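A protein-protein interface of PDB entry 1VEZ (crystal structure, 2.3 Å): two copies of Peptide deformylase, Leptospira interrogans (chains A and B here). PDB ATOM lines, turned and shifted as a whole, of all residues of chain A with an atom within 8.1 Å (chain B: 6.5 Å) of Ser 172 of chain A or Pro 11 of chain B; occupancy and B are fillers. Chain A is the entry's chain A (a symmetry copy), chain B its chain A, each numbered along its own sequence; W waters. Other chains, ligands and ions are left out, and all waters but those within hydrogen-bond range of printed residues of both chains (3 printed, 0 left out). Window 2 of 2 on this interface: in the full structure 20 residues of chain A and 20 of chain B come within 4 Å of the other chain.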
ATOM      1  N   LYS A 161       3.687  36.520 -13.810  1.00  0.00           N
ATOM      2  CA  LYS A 161       2.579  35.723 -13.275  1.00  0.00           C
ATOM      3  C   LYS A 161       1.568  35.466 -14.394  1.00  0.00           C
ATOM      4  O   LYS A 161       0.822  34.496 -14.354  1.00  0.00           O
ATOM      5  CB  LYS A 161       1.862  36.447 -12.127  1.00  0.00           C
ATOM      6  CG  LYS A 161       2.681  36.609 -10.860  1.00  0.00           C
ATOM      7  CD  LYS A 161       1.901  37.401  -9.813  1.00  0.00           C
ATOM      8  CE  LYS A 161       2.739  37.639  -8.558  1.00  0.00           C
ATOM      9  NZ  LYS A 161       1.997  38.369  -7.470  1.00  0.00           N
ATOM     10  N   PHE A 165       1.903  27.658 -19.560  1.00  0.00           N
ATOM     11  CA  PHE A 165       1.708  26.668 -20.603  1.00  0.00           C
ATOM     12  C   PHE A 165       0.250  26.649 -21.050  1.00  0.00           C
ATOM     13  O   PHE A 165      -0.669  26.717 -20.224  1.00  0.00           O
ATOM     14  CB  PHE A 165       2.141  25.287 -20.104  1.00  0.00           C
ATOM     15  CG  PHE A 165       3.592  25.217 -19.737  1.00  0.00           C
ATOM     16  CD1 PHE A 165       4.029  25.664 -18.495  1.00  0.00           C
ATOM     17  CD2 PHE A 165       4.531  24.771 -20.658  1.00  0.00           C
ATOM     18  CE1 PHE A 165       5.381  25.671 -18.176  1.00  0.00           C
ATOM     19  CE2 PHE A 165       5.884  24.776 -20.350  1.00  0.00           C
ATOM     20  CZ  PHE A 165       6.312  25.227 -19.107  1.00  0.00           C
ATOM     21  N   ASN A 166       0.064  26.569 -22.367  1.00  0.00           N
ATOM     22  CA  ASN A 166      -1.247  26.561 -23.013  1.00  0.00           C
ATOM     23  C   ASN A 166      -2.346  25.756 -22.350  1.00  0.00           C
ATOM     24  O   ASN A 166      -3.349  26.314 -21.910  1.00  0.00           O
ATOM     25  CB  ASN A 166      -1.108  26.070 -24.450  1.00  0.00           C
ATOM     26  CG  ASN A 166      -0.279  26.993 -25.296  1.00  0.00           C
ATOM     27  OD1 ASN A 166       0.112  26.645 -26.406  1.00  0.00           O
ATOM     28  ND2 ASN A 166      -0.003  28.185 -24.779  1.00  0.00           N
ATOM     29  N   GLU A 167      -2.164  24.441 -22.306  1.00  0.00           N
ATOM     30  CA  GLU A 167      -3.158  23.551 -21.725  1.00  0.00           C
ATOM     31  C   GLU A 167      -3.566  23.927 -20.310  1.00  0.00           C
ATOM     32  O   GLU A 167      -4.697  23.668 -19.904  1.00  0.00           O
ATOM     33  CB  GLU A 167      -2.653  22.106 -21.753  1.00  0.00           C
ATOM     34  CG  GLU A 167      -2.502  21.567 -23.168  1.00  0.00           C
ATOM     35  N   THR A 168      -2.651  24.539 -19.564  1.00  0.00           N
ATOM     36  CA  THR A 168      -2.930  24.948 -18.189  1.00  0.00           C
ATOM     37  C   THR A 168      -3.678  26.273 -18.171  1.00  0.00           C
ATOM     38  O   THR A 168      -4.622  26.455 -17.409  1.00  0.00           O
ATOM     39  CB  THR A 168      -1.631  25.117 -17.376  1.00  0.00           C
ATOM     40  OG1 THR A 168      -0.831  23.935 -17.498  1.00  0.00           O
ATOM     41  CG2 THR A 168      -1.948  25.341 -15.914  1.00  0.00           C
ATOM     42  N   LEU A 169      -3.241  27.208 -19.003  1.00  0.00           N
ATOM     43  CA  LEU A 169      -3.894  28.504 -19.070  1.00  0.00           C
ATOM     44  C   LEU A 169      -5.320  28.318 -19.562  1.00  0.00           C
ATOM     45  O   LEU A 169      -6.240  28.976 -19.080  1.00  0.00           O
ATOM     46  CB  LEU A 169      -3.141  29.434 -20.022  1.00  0.00           C
ATOM     47  CG  LEU A 169      -1.776  29.938 -19.556  1.00  0.00           C
ATOM     48  CD1 LEU A 169      -1.084  30.647 -20.689  1.00  0.00           C
ATOM     49  CD2 LEU A 169      -1.947  30.865 -18.362  1.00  0.00           C
ATOM     50  N   ASP A 170      -5.496  27.414 -20.523  1.00  0.00           N
ATOM     51  CA  ASP A 170      -6.809  27.135 -21.090  1.00  0.00           C
ATOM     52  C   ASP A 170      -7.772  26.582 -20.037  1.00  0.00           C
ATOM     53  O   ASP A 170      -8.960  26.915 -20.038  1.00  0.00           O
ATOM     54  CB  ASP A 170      -6.677  26.153 -22.253  1.00  0.00           C
ATOM     55  N   SER A 171      -7.255  25.747 -19.138  1.00  0.00           N
ATOM     56  CA  SER A 171      -8.065  25.146 -18.076  1.00  0.00           C
ATOM     57  C   SER A 171      -8.223  26.080 -16.873  1.00  0.00           C
ATOM     58  O   SER A 171      -8.800  25.692 -15.853  1.00  0.00           O
ATOM     59  CB  SER A 171      -7.428  23.835 -17.601  1.00  0.00           C
ATOM     60  OG  SER A 171      -7.205  22.943 -18.680  1.00  0.00           O
ATOM     61  N   SER A 172      -7.716  27.304 -16.993  1.00  0.00           N
ATOM     62  CA  SER A 172      -7.786  28.273 -15.900  1.00  0.00           C
ATOM     63  C   SER A 172      -8.155  29.671 -16.393  1.00  0.00           C
ATOM     64  O   SER A 172      -8.426  29.821 -17.606  1.00  0.00           O
ATOM     65  CB  SER A 172      -6.439  28.330 -15.164  1.00  0.00           C
ATOM     66  OG  SER A 172      -6.052  27.051 -14.672  1.00  0.00           O
ATOM     67  N   ARG B   7       1.596  22.885 -13.683  1.00  0.00           N
ATOM     68  CA  ARG B   7       2.461  23.672 -14.557  1.00  0.00           C
ATOM     69  C   ARG B   7       2.223  25.162 -14.395  1.00  0.00           C
ATOM     70  O   ARG B   7       1.134  25.595 -14.012  1.00  0.00           O
ATOM     71  CB  ARG B   7       2.191  23.333 -16.019  1.00  0.00           C
ATOM     72  CG  ARG B   7       2.125  21.866 -16.350  1.00  0.00           C
ATOM     73  CD  ARG B   7       3.448  21.379 -16.857  1.00  0.00           C
ATOM     74  NE  ARG B   7       3.285  20.271 -17.794  1.00  0.00           N
ATOM     75  CZ  ARG B   7       2.657  20.364 -18.966  1.00  0.00           C
ATOM     76  NH1 ARG B   7       2.126  21.521 -19.353  1.00  0.00           N
ATOM     77  NH2 ARG B   7       2.566  19.296 -19.754  1.00  0.00           N
ATOM     78  N   GLY B   9       1.058  28.598 -14.957  1.00  0.00           N
ATOM     79  CA  GLY B   9      -0.160  28.955 -15.655  1.00  0.00           C
ATOM     80  C   GLY B   9      -1.312  28.628 -14.726  1.00  0.00           C
ATOM     81  O   GLY B   9      -2.348  29.293 -14.738  1.00  0.00           O
ATOM     82  N   ASP B  10      -1.133  27.587 -13.914  1.00  0.00           N
ATOM     83  CA  ASP B  10      -2.149  27.201 -12.943  1.00  0.00           C
ATOM     84  C   ASP B  10      -2.069  28.253 -11.842  1.00  0.00           C
ATOM     85  O   ASP B  10      -1.019  28.435 -11.229  1.00  0.00           O
ATOM     86  CB  ASP B  10      -1.835  25.831 -12.349  1.00  0.00           C
ATOM     87  CG  ASP B  10      -2.978  25.281 -11.522  1.00  0.00           C
ATOM     88  OD1 ASP B  10      -3.439  25.969 -10.593  1.00  0.00           O
ATOM     89  OD2 ASP B  10      -3.417  24.154 -11.811  1.00  0.00           O
ATOM     90  N   PRO B  11      -3.173  28.964 -11.578  1.00  0.00           N
ATOM     91  CA  PRO B  11      -3.138  29.991 -10.531  1.00  0.00           C
ATOM     92  C   PRO B  11      -2.761  29.510  -9.128  1.00  0.00           C
ATOM     93  O   PRO B  11      -2.363  30.311  -8.280  1.00  0.00           O
ATOM     94  CB  PRO B  11      -4.538  30.612 -10.602  1.00  0.00           C
ATOM     95  CG  PRO B  11      -5.380  29.523 -11.175  1.00  0.00           C
ATOM     96  CD  PRO B  11      -4.496  28.899 -12.217  1.00  0.00           C
ATOM     97  N   ILE B  12      -2.870  28.208  -8.884  1.00  0.00           N
ATOM     98  CA  ILE B  12      -2.520  27.672  -7.571  1.00  0.00           C
ATOM     99  C   ILE B  12      -1.054  27.978  -7.261  1.00  0.00           C
ATOM    100  O   ILE B  12      -0.713  28.347  -6.140  1.00  0.00           O
ATOM    101  CB  ILE B  12      -2.725  26.141  -7.497  1.00  0.00           C
ATOM    102  CG1 ILE B  12      -4.188  25.783  -7.779  1.00  0.00           C
ATOM    103  CG2 ILE B  12      -2.325  25.634  -6.117  1.00  0.00           C
ATOM    104  CD1 ILE B  12      -5.180  26.428  -6.833  1.00  0.00           C
ATOM    105  N   LEU B  13      -0.195  27.838  -8.267  1.00  0.00           N
ATOM    106  CA  LEU B  13       1.231  28.087  -8.103  1.00  0.00           C
ATOM    107  C   LEU B  13       1.575  29.522  -7.722  1.00  0.00           C
ATOM    108  O   LEU B  13       2.708  29.803  -7.337  1.00  0.00           O
ATOM    109  CB  LEU B  13       1.976  27.712  -9.386  1.00  0.00           C
ATOM    110  CG  LEU B  13       1.942  26.230  -9.761  1.00  0.00           C
ATOM    111  CD1 LEU B  13       2.674  25.994 -11.083  1.00  0.00           C
ATOM    112  CD2 LEU B  13       2.589  25.425  -8.635  1.00  0.00           C
ATOM    113  N   ARG B  14       0.611  30.434  -7.837  1.00  0.00           N
ATOM    114  CA  ARG B  14       0.857  31.828  -7.489  1.00  0.00           C
ATOM    115  C   ARG B  14       0.172  32.234  -6.193  1.00  0.00           C
ATOM    116  O   ARG B  14       0.256  33.387  -5.771  1.00  0.00           O
ATOM    117  CB  ARG B  14       0.417  32.757  -8.627  1.00  0.00           C
ATOM    118  CG  ARG B  14       1.532  33.125  -9.605  1.00  0.00           C
ATOM    119  CD  ARG B  14       2.214  31.895 -10.194  1.00  0.00           C
ATOM    120  NE  ARG B  14       3.177  32.249 -11.232  1.00  0.00           N
ATOM    121  CZ  ARG B  14       4.301  32.923 -11.022  1.00  0.00           C
ATOM    122  NH1 ARG B  14       4.626  33.323  -9.797  1.00  0.00           N
ATOM    123  NH2 ARG B  14       5.095  33.209 -12.044  1.00  0.00           N
ATOM    124  N   LYS B  15      -0.512  31.286  -5.564  1.00  0.00           N
ATOM    125  CA  LYS B  15      -1.189  31.564  -4.298  1.00  0.00           C
ATOM    126  C   LYS B  15      -0.219  31.317  -3.141  1.00  0.00           C
ATOM    127  O   LYS B  15       0.813  30.676  -3.307  1.00  0.00           O
ATOM    128  CB  LYS B  15      -2.423  30.676  -4.154  1.00  0.00           C
ATOM    129  CG  LYS B  15      -3.504  30.943  -5.191  1.00  0.00           C
ATOM    130  CD  LYS B  15      -4.629  29.922  -5.066  1.00  0.00           C
ATOM    131  CE  LYS B  15      -5.695  30.124  -6.123  1.00  0.00           C
ATOM    132  NZ  LYS B  15      -6.355  31.440  -5.951  1.00  0.00           N
HETATM  133  O   HOH W   1       3.104  32.620 -14.172  1.00  0.00           O
HETATM  134  O   HOH W   2      -0.879  22.035 -14.716  1.00  0.00           O
HETATM  135  O   HOH W   3       0.285  22.416 -21.187  1.00  0.00           O
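The side-chain carboxylate (OD1) of Asp 10 of chain B lies within hydrogen-bond range of the backbone NH (N) of Ile 12 of chain B (2.9 Å).
OG of Ser 172 of chain A is in hydrogen-bond range of O of Thr 168 of chain A (3.1 Å).
Lys 161 of chain A touches Arg 14 of chain B.
Phe 165 of chain A touches Arg 7 of chain B.
Thr 168 of chain A touches Arg 7 of chain B.
Thr 168 of chain A touches Gly 9 of chain B (CG2 to C, 3.6 Å).
Asp 10 of chain B touches Thr 168 of chain A (N to CG2, 3.1 Å).
Leu 169 of chain A touches Gly 9 of chain B (CD2 to CA, 3.8 Å).
Ser 172 of chain A touches Pro 11 of chain B.
Pro 11 of chain B touches just one residue of chain A: Ser 172 (3.4 Å).
Of the printed residues of chain A, Arg 7 of chain B touches Phe 165 (3.8 Å) and Thr 168 (3.4 Å).
Printed residues of chain B within 4 Å of Thr 168 of chain A: Arg 7, Gly 9 and Asp 10.
Printed residues of chain A within 4 Å of Arg 14 of chain B: Lys 161.
Printed residues of chain B within 4 Å of Phe 165 of chain A: Arg 7 (3.8 Å).
Printed residues of chain B within 4 Å of Lys 161 of chain A: Arg 14 (3.8 Å).
The nearest residue of chain B that does not touch Ser 172 of chain A is Gly 9 of chain B (4.2 Å).
The nearest residue of chain A that does not touch Pro 11 of chain B is Thr 168 of chain A (5.7 Å).
Hydrophobic or aromatic side chains of chain B that line the printed part of chain A: Pro 11.
Of the 9 printed residues of chain A, 5 touch a printed residue of chain B.
Hydrophobic or aromatic side chains of chain A within 4 Å of the printed part of chain B: Phe 165 and Leu 169.
No position is printed for both chains.
Of the 7 pairs that touch across the chains among the printed residues, none has its exchanged pair printed and touching as well.
Water W3 bridges the guanidinium group of Arg 7 of chain B (2.7 Å) and the backbone NH of Glu 167 of chain A (3.4 Å).
Water W2 bridges the backbone NH of Arg 7 of chain B (2.8 Å) and the side-chain hydroxyl of Thr 168 of chain A (3.4 Å).
Water W1 bridges O of Lys 161 of chain A (3.0 Å) and NE of Arg 14 of chain B (3.0 Å).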
